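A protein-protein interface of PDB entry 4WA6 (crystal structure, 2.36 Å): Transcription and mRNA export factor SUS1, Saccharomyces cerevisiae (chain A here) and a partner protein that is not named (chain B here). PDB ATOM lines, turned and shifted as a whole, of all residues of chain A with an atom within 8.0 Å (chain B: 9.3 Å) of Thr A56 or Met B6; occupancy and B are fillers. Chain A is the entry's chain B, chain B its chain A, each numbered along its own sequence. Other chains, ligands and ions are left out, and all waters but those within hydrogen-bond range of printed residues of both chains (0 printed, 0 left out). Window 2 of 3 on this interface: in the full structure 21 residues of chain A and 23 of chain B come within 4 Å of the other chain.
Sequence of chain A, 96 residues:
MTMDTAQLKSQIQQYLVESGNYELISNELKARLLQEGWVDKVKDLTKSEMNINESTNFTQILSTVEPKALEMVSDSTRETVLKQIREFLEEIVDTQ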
ATOM      1  N   GLU A  49       1.936 -23.837  24.984  1.00  0.00           N
ATOM      2  CA  GLU A  49       2.167 -25.141  24.377  1.00  0.00           C
ATOM      3  C   GLU A  49       3.358 -25.162  23.451  1.00  0.00           C
ATOM      4  O   GLU A  49       4.047 -26.179  23.417  1.00  0.00           O
ATOM      5  CB  GLU A  49       0.928 -25.701  23.666  1.00  0.00           C
ATOM      6  CG  GLU A  49      -0.249 -26.011  24.584  1.00  0.00           C
ATOM      7  CD  GLU A  49      -0.092 -27.274  25.428  1.00  0.00           C
ATOM      8  OE1 GLU A  49       0.623 -28.244  25.047  1.00  0.00           O
ATOM      9  OE2 GLU A  49      -0.722 -27.293  26.502  1.00  0.00           O
ATOM     10  N   MET A  50       3.632 -24.086  22.719  1.00  0.00           N
ATOM     11  CA  MET A  50       4.922 -23.990  22.014  1.00  0.00           C
ATOM     12  C   MET A  50       6.115 -24.057  22.971  1.00  0.00           C
ATOM     13  O   MET A  50       7.108 -24.728  22.667  1.00  0.00           O
ATOM     14  CB  MET A  50       5.060 -22.742  21.143  1.00  0.00           C
ATOM     15  CG  MET A  50       4.113 -22.713  19.946  1.00  0.00           C
ATOM     16  SD  MET A  50       4.457 -21.327  18.837  1.00  0.00           S
ATOM     17  CE  MET A  50       3.965 -19.974  19.927  1.00  0.00           C
ATOM     18  N   ASN A  51       6.025 -23.371  24.103  1.00  0.00           N
ATOM     19  CA  ASN A  51       7.169 -23.241  24.998  1.00  0.00           C
ATOM     20  C   ASN A  51       7.495 -24.583  25.643  1.00  0.00           C
ATOM     21  O   ASN A  51       8.648 -25.054  25.578  1.00  0.00           O
ATOM     22  CB  ASN A  51       6.926 -22.178  26.073  1.00  0.00           C
ATOM     23  CG  ASN A  51       7.057 -20.765  25.532  1.00  0.00           C
ATOM     24  OD1 ASN A  51       7.758 -20.514  24.537  1.00  0.00           O
ATOM     25  ND2 ASN A  51       6.385 -19.822  26.188  1.00  0.00           N
ATOM     26  N   ASN A  53       6.480 -27.602  24.667  1.00  0.00           N
ATOM     27  CA  ASN A  53       6.913 -28.618  23.696  1.00  0.00           C
ATOM     28  C   ASN A  53       8.139 -28.188  22.880  1.00  0.00           C
ATOM     29  O   ASN A  53       8.595 -28.950  22.028  1.00  0.00           O
ATOM     30  CB  ASN A  53       5.763 -29.018  22.783  1.00  0.00           C
ATOM     31  CG  ASN A  53       4.682 -29.768  23.525  1.00  0.00           C
ATOM     32  OD1 ASN A  53       4.839 -30.960  23.789  1.00  0.00           O
ATOM     33  ND2 ASN A  53       3.577 -29.096  23.855  1.00  0.00           N
ATOM     34  N   GLU A  54       8.692 -27.006  23.171  1.00  0.00           N
ATOM     35  CA  GLU A  54       9.831 -26.478  22.418  1.00  0.00           C
ATOM     36  C   GLU A  54       9.617 -26.847  20.965  1.00  0.00           C
ATOM     37  O   GLU A  54      10.469 -27.503  20.359  1.00  0.00           O
ATOM     38  CB  GLU A  54      11.176 -27.019  22.927  1.00  0.00           C
ATOM     39  CG  GLU A  54      11.662 -26.355  24.205  1.00  0.00           C
ATOM     40  CD  GLU A  54      12.918 -27.009  24.850  1.00  0.00           C
ATOM     41  OE1 GLU A  54      13.284 -28.185  24.539  1.00  0.00           O
ATOM     42  OE2 GLU A  54      13.552 -26.322  25.702  1.00  0.00           O
ATOM     43  N   SER A  55       8.461 -26.440  20.423  1.00  0.00           N
ATOM     44  CA  SER A  55       8.146 -26.688  19.024  1.00  0.00           C
ATOM     45  C   SER A  55       7.240 -25.611  18.429  1.00  0.00           C
ATOM     46  O   SER A  55       6.411 -25.064  19.137  1.00  0.00           O
ATOM     47  CB  SER A  55       7.499 -28.056  18.868  1.00  0.00           C
ATOM     48  OG  SER A  55       7.103 -28.274  17.524  1.00  0.00           O
ATOM     49  N   THR A  56       7.440 -25.309  17.147  1.00  0.00           N
ATOM     50  CA  THR A  56       6.567 -24.436  16.416  1.00  0.00           C
ATOM     51  C   THR A  56       5.820 -25.183  15.330  1.00  0.00           C
ATOM     52  O   THR A  56       5.142 -24.561  14.512  1.00  0.00           O
ATOM     53  CB  THR A  56       7.318 -23.249  15.767  1.00  0.00           C
ATOM     54  OG1 THR A  56       8.128 -23.717  14.685  1.00  0.00           O
ATOM     55  CG2 THR A  56       8.160 -22.557  16.788  1.00  0.00           C
ATOM     56  N   ASN A  57       5.912 -26.504  15.329  1.00  0.00           N
ATOM     57  CA  ASN A  57       5.243 -27.295  14.303  1.00  0.00           C
ATOM     58  C   ASN A  57       3.745 -27.238  14.498  1.00  0.00           C
ATOM     59  O   ASN A  57       3.217 -27.649  15.534  1.00  0.00           O
ATOM     60  CB  ASN A  57       5.727 -28.759  14.302  1.00  0.00           C
ATOM     61  CG  ASN A  57       4.912 -29.631  13.337  1.00  0.00           C
ATOM     62  OD1 ASN A  57       3.789 -30.031  13.633  1.00  0.00           O
ATOM     63  ND2 ASN A  57       5.437 -29.842  12.151  1.00  0.00           N
ATOM     64  N   PHE A  58       3.068 -26.696  13.481  1.00  0.00           N
ATOM     65  CA  PHE A  58       1.672 -26.412  13.564  1.00  0.00           C
ATOM     66  C   PHE A  58       0.913 -27.659  14.041  1.00  0.00           C
ATOM     67  O   PHE A  58       0.089 -27.609  14.941  1.00  0.00           O
ATOM     68  CB  PHE A  58       1.122 -25.927  12.202  1.00  0.00           C
ATOM     69  CG  PHE A  58      -0.351 -25.796  12.202  1.00  0.00           C
ATOM     70  CD1 PHE A  58      -0.950 -24.711  12.834  1.00  0.00           C
ATOM     71  CD2 PHE A  58      -1.144 -26.821  11.720  1.00  0.00           C
ATOM     72  CE1 PHE A  58      -2.305 -24.638  12.934  1.00  0.00           C
ATOM     73  CE2 PHE A  58      -2.525 -26.741  11.794  1.00  0.00           C
ATOM     74  CZ  PHE A  58      -3.109 -25.657  12.410  1.00  0.00           C
ATOM     75  N   THR A  59       1.217 -28.794  13.462  1.00  0.00           N
ATOM     76  CA  THR A  59       0.348 -30.007  13.613  1.00  0.00           C
ATOM     77  C   THR A  59       0.482 -30.531  15.025  1.00  0.00           C
ATOM     78  O   THR A  59      -0.482 -30.750  15.736  1.00  0.00           O
ATOM     79  CB  THR A  59       0.758 -31.046  12.576  1.00  0.00           C
ATOM     80  OG1 THR A  59       0.507 -30.518  11.254  1.00  0.00           O
ATOM     81  CG2 THR A  59       0.054 -32.364  12.778  1.00  0.00           C
ATOM     82  N   GLN A  60       1.717 -30.644  15.456  1.00  0.00           N
ATOM     83  CA  GLN A  60       1.997 -30.994  16.803  1.00  0.00           C
ATOM     84  C   GLN A  60       1.300 -30.040  17.802  1.00  0.00           C
ATOM     85  O   GLN A  60       0.635 -30.483  18.754  1.00  0.00           O
ATOM     86  CB  GLN A  60       3.496 -31.015  16.987  1.00  0.00           C
ATOM     87  CG  GLN A  60       3.888 -31.293  18.405  1.00  0.00           C
ATOM     88  CD  GLN A  60       5.387 -31.297  18.592  1.00  0.00           C
ATOM     89  OE1 GLN A  60       6.149 -31.022  17.649  1.00  0.00           O
ATOM     90  NE2 GLN A  60       5.831 -31.617  19.812  1.00  0.00           N
ATOM     91  N   ILE A  61       1.416 -28.743  17.579  1.00  0.00           N
ATOM     92  CA  ILE A  61       0.919 -27.783  18.549  1.00  0.00           C
ATOM     93  C   ILE A  61      -0.605 -27.767  18.625  1.00  0.00           C
ATOM     94  O   ILE A  61      -1.201 -27.748  19.712  1.00  0.00           O
ATOM     95  CB  ILE A  61       1.483 -26.404  18.220  1.00  0.00           C
ATOM     96  CG1 ILE A  61       2.998 -26.418  18.454  1.00  0.00           C
ATOM     97  CG2 ILE A  61       0.823 -25.309  19.036  1.00  0.00           C
ATOM     98  CD1 ILE A  61       3.442 -26.728  19.884  1.00  0.00           C
ATOM     99  N   LEU A  62      -1.229 -27.855  17.469  1.00  0.00           N
ATOM    100  CA  LEU A  62      -2.668 -27.881  17.405  1.00  0.00           C
ATOM    101  C   LEU A  62      -3.167 -29.078  18.133  1.00  0.00           C
ATOM    102  O   LEU A  62      -4.215 -29.050  18.784  1.00  0.00           O
ATOM    103  CB  LEU A  62      -3.106 -28.017  15.935  1.00  0.00           C
ATOM    104  CG  LEU A  62      -4.576 -28.036  15.647  1.00  0.00           C
ATOM    105  CD1 LEU A  62      -5.038 -26.603  15.901  1.00  0.00           C
ATOM    106  CD2 LEU A  62      -4.914 -28.528  14.232  1.00  0.00           C
ATOM    107  N   MET B   6      16.486 -23.994  13.214  1.00  0.00           N
ATOM    108  CA  MET B   6      15.188 -23.963  12.452  1.00  0.00           C
ATOM    109  C   MET B   6      15.369 -24.274  10.957  1.00  0.00           C
ATOM    110  O   MET B   6      16.245 -23.735  10.268  1.00  0.00           O
ATOM    111  CB  MET B   6      14.444 -22.629  12.630  1.00  0.00           C
ATOM    112  CG  MET B   6      13.869 -22.421  14.023  1.00  0.00           C
ATOM    113  SD  MET B   6      12.295 -23.220  14.450  1.00  0.00           S
ATOM    114  CE  MET B   6      11.195 -22.827  13.083  1.00  0.00           C
ATOM    115  N   SER B   7      14.518 -25.160  10.466  1.00  0.00           N
ATOM    116  CA  SER B   7      14.617 -25.636   9.104  1.00  0.00           C
ATOM    117  C   SER B   7      13.675 -24.798   8.265  1.00  0.00           C
ATOM    118  O   SER B   7      12.681 -24.291   8.767  1.00  0.00           O
ATOM    119  CB  SER B   7      14.194 -27.107   9.040  1.00  0.00           C
ATOM    120  OG  SER B   7      12.838 -27.249   9.505  1.00  0.00           O
ATOM    121  N   ILE B   8      14.029 -24.634   6.998  1.00  0.00           N
ATOM    122  CA  ILE B   8      13.121 -24.163   5.983  1.00  0.00           C
ATOM    123  C   ILE B   8      12.589 -25.403   5.298  1.00  0.00           C
ATOM    124  O   ILE B   8      13.229 -26.407   5.285  1.00  0.00           O
ATOM    125  CB  ILE B   8      13.849 -23.239   5.003  1.00  0.00           C
ATOM    126  CG1 ILE B   8      14.068 -21.859   5.669  1.00  0.00           C
ATOM    127  CG2 ILE B   8      13.088 -23.108   3.698  1.00  0.00           C
ATOM    128  CD1 ILE B   8      15.405 -21.753   6.398  1.00  0.00           C
ATOM    129  N   CYS B   9      11.382 -25.369   4.779  1.00  0.00           N
ATOM    130  CA  CYS B   9      10.816 -26.554   4.148  1.00  0.00           C
ATOM    131  C   CYS B   9      11.686 -26.878   2.937  1.00  0.00           C
ATOM    132  O   CYS B   9      12.025 -25.988   2.168  1.00  0.00           O
ATOM    133  CB  CYS B   9       9.357 -26.293   3.743  1.00  0.00           C
ATOM    134  SG  CYS B   9       8.756 -27.243   2.356  1.00  0.00           S
ATOM    135  N   GLN B  13      11.872 -25.428  -1.255  1.00  0.00           N
ATOM    136  CA  GLN B  13      13.255 -25.158  -1.760  1.00  0.00           C
ATOM    137  C   GLN B  13      13.550 -25.857  -3.069  1.00  0.00           C
ATOM    138  O   GLN B  13      14.170 -25.278  -3.950  1.00  0.00           O
ATOM    139  CB  GLN B  13      14.319 -25.585  -0.749  1.00  0.00           C
ATOM    140  CG  GLN B  13      14.402 -24.659   0.442  1.00  0.00           C
ATOM    141  CD  GLN B  13      15.641 -24.861   1.269  1.00  0.00           C
ATOM    142  OE1 GLN B  13      16.447 -25.738   1.010  1.00  0.00           O
ATOM    143  NE2 GLN B  13      15.811 -24.028   2.263  1.00  0.00           N
ATOM    144  N   PHE B 100       0.704 -23.949   3.365  1.00  0.00           N
ATOM    145  CA  PHE B 100       0.968 -25.189   4.090  1.00  0.00           C
ATOM    146  C   PHE B 100       1.597 -26.308   3.246  1.00  0.00           C
ATOM    147  O   PHE B 100       1.215 -26.530   2.112  1.00  0.00           O
ATOM    148  CB  PHE B 100      -0.304 -25.678   4.724  1.00  0.00           C
ATOM    149  CG  PHE B 100      -0.106 -26.629   5.833  1.00  0.00           C
ATOM    150  CD1 PHE B 100      -0.045 -27.971   5.589  1.00  0.00           C
ATOM    151  CD2 PHE B 100      -0.007 -26.171   7.136  1.00  0.00           C
ATOM    152  CE1 PHE B 100       0.114 -28.866   6.644  1.00  0.00           C
ATOM    153  CE2 PHE B 100       0.152 -27.041   8.201  1.00  0.00           C
ATOM    154  CZ  PHE B 100       0.201 -28.395   7.963  1.00  0.00           C
ATOM    155  N   CYS B 104       5.939 -31.660   5.142  1.00  0.00           N
ATOM    156  CA  CYS B 104       6.351 -31.169   6.474  1.00  0.00           C
ATOM    157  C   CYS B 104       5.223 -31.151   7.532  1.00  0.00           C
ATOM    158  O   CYS B 104       5.508 -31.095   8.717  1.00  0.00           O
ATOM    159  CB  CYS B 104       6.912 -29.767   6.370  1.00  0.00           C
ATOM    160  SG  CYS B 104       8.432 -29.587   5.428  1.00  0.00           S
ATOM    161  N   GLU B 105       3.946 -31.192   7.134  1.00  0.00           N
ATOM    162  CA  GLU B 105       2.847 -31.038   8.093  1.00  0.00           C
ATOM    163  C   GLU B 105       3.006 -29.729   8.910  1.00  0.00           C
ATOM    164  O   GLU B 105       2.814 -29.673  10.145  1.00  0.00           O
ATOM    165  CB  GLU B 105       2.751 -32.253   8.999  1.00  0.00           C
ATOM    166  CG  GLU B 105       2.865 -33.553   8.220  1.00  0.00           C
ATOM    167  CD  GLU B 105       2.699 -34.809   9.061  1.00  0.00           C
ATOM    168  OE1 GLU B 105       3.209 -35.846   8.602  1.00  0.00           O
ATOM    169  OE2 GLU B 105       2.081 -34.789  10.157  1.00  0.00           O
ATOM    170  N   ASP B 106       3.292 -28.662   8.183  1.00  0.00           N
ATOM    171  CA  ASP B 106       3.534 -27.383   8.778  1.00  0.00           C
ATOM    172  C   ASP B 106       3.358 -26.279   7.759  1.00  0.00           C
ATOM    173  O   ASP B 106       3.387 -26.506   6.552  1.00  0.00           O
ATOM    174  CB  ASP B 106       4.977 -27.318   9.318  1.00  0.00           C
ATOM    175  CG  ASP B 106       5.122 -26.349  10.496  1.00  0.00           C
ATOM    176  OD1 ASP B 106       4.097 -25.837  10.998  1.00  0.00           O
ATOM    177  OD2 ASP B 106       6.248 -26.144  10.967  1.00  0.00           O
ATOM    178  N   TYR B 107       3.164 -25.080   8.282  1.00  0.00           N
ATOM    179  CA  TYR B 107       3.112 -23.886   7.488  1.00  0.00           C
ATOM    180  C   TYR B 107       4.536 -23.519   7.131  1.00  0.00           C
ATOM    181  O   TYR B 107       5.443 -23.681   7.933  1.00  0.00           O
ATOM    182  CB  TYR B 107       2.451 -22.747   8.263  1.00  0.00           C
ATOM    183  CG  TYR B 107       0.946 -22.878   8.271  1.00  0.00           C
ATOM    184  CD1 TYR B 107       0.192 -22.510   7.163  1.00  0.00           C
ATOM    185  CD2 TYR B 107       0.295 -23.466   9.346  1.00  0.00           C
ATOM    186  CE1 TYR B 107      -1.200 -22.699   7.142  1.00  0.00           C
ATOM    187  CE2 TYR B 107      -1.075 -23.639   9.345  1.00  0.00           C
ATOM    188  CZ  TYR B 107      -1.816 -23.241   8.247  1.00  0.00           C
ATOM    189  OH  TYR B 107      -3.156 -23.428   8.270  1.00  0.00           O
ATOM    190  N   ILE B 108       4.713 -23.045   5.919  1.00  0.00           N
ATOM    191  CA  ILE B 108       5.906 -22.369   5.501  1.00  0.00           C
ATOM    192  C   ILE B 108       5.792 -20.883   5.875  1.00  0.00           C
ATOM    193  O   ILE B 108       5.158 -20.083   5.171  1.00  0.00           O
ATOM    194  CB  ILE B 108       6.046 -22.530   3.999  1.00  0.00           C
ATOM    195  CG1 ILE B 108       6.088 -24.025   3.661  1.00  0.00           C
ATOM    196  CG2 ILE B 108       7.314 -21.859   3.521  1.00  0.00           C
ATOM    197  CD1 ILE B 108       5.969 -24.272   2.178  1.00  0.00           C
ATOM    198  N   GLY B 109       6.412 -20.508   6.987  1.00  0.00           N
ATOM    199  CA  GLY B 109       6.214 -19.178   7.541  1.00  0.00           C
ATOM    200  C   GLY B 109       7.428 -18.287   7.493  1.00  0.00           C
ATOM    201  O   GLY B 109       7.351 -17.086   7.728  1.00  0.00           O
ATOM    202  N   ASN B 110       8.561 -18.868   7.145  1.00  0.00           N
ATOM    203  CA  ASN B 110       9.834 -18.258   7.474  1.00  0.00           C
ATOM    204  C   ASN B 110      10.616 -17.997   6.214  1.00  0.00           C
ATOM    205  O   ASN B 110      11.823 -17.957   6.236  1.00  0.00           O
ATOM    206  CB  ASN B 110      10.581 -19.147   8.473  1.00  0.00           C
ATOM    207  CG  ASN B 110      10.787 -20.561   7.953  1.00  0.00           C
ATOM    208  OD1 ASN B 110      10.440 -20.844   6.794  1.00  0.00           O
ATOM    209  ND2 ASN B 110      11.375 -21.453   8.792  1.00  0.00           N
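Among the printed residues, merely in contact across the chains: Thr A56 with Met B6, Phe A58 with Tyr B107, Asn A57 with Cys B104, Asn A57 with Asp B106, Phe A58 with Phe B100, Thr A56 with Asp B106 and Thr A59 with Phe B100.
Thr A56 touches just these residues of chain B: Met B6 and Asp B106. Met B6 touches one residue of chain A. No residue of chain B comes within 4 Å of Ser A55. Of the printed residues of chain B, Thr A59 touches Phe B100 and Glu B105. Of the printed residues of chain B, Asn A57 touches Cys B104 (3.7 Å), Glu B105 (3.3 Å) and Asp B106 (3.7 Å). Of the printed residues of chain A, Cys B104 touches Asn A57 (3.7 Å). Printed residues of chain A within 4 Å of Tyr B107: Phe A58. Printed residues of chain A within 4 Å of Phe B100: Phe A58 and Thr A59. Ile B8 touches none of the printed residues of chain A. Glu A49 touches none of the printed residues of chain B. The nearest residue of chain A that does not touch Met B6 is Asn A57 (6.8 Å). The nearest printed residue of chain A that does not touch Phe B100 is Asn A57 (6.9 Å).
Among the printed residues, 10 pairs touch across the chains. Among the printed residues, no Asp or Glu carboxylate lies within 4 Å of a Lys or Arg side-chain nitrogen of the other chain.
The backbone NH (N) of Gln A60 is in hydrogen-bond range of the side-chain amide oxygen (OD1) of Asn A57, 2.8 Å away. OD1 of Asn A57 is in hydrogen-bond range of N of Thr A59, 2.9 Å away. The side-chain hydroxyl (OG) of Ser A55 sits at hydrogen-bond distance from the backbone NH (N) of Asn A57 (3.1 Å).
The backbone carbonyl oxygen (O) of Glu B105 is in hydrogen-bond range of the side-chain hydroxyl (OG1) of Thr A59 (2.7 Å). ND2 of Asn A57 is in hydrogen-bond range of O of Glu B105 (3.3 Å). The backbone NH (N) of Phe A58 is in hydrogen-bond range of the side-chain carboxylate (OD1) of Asp B106 (2.8 Å).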
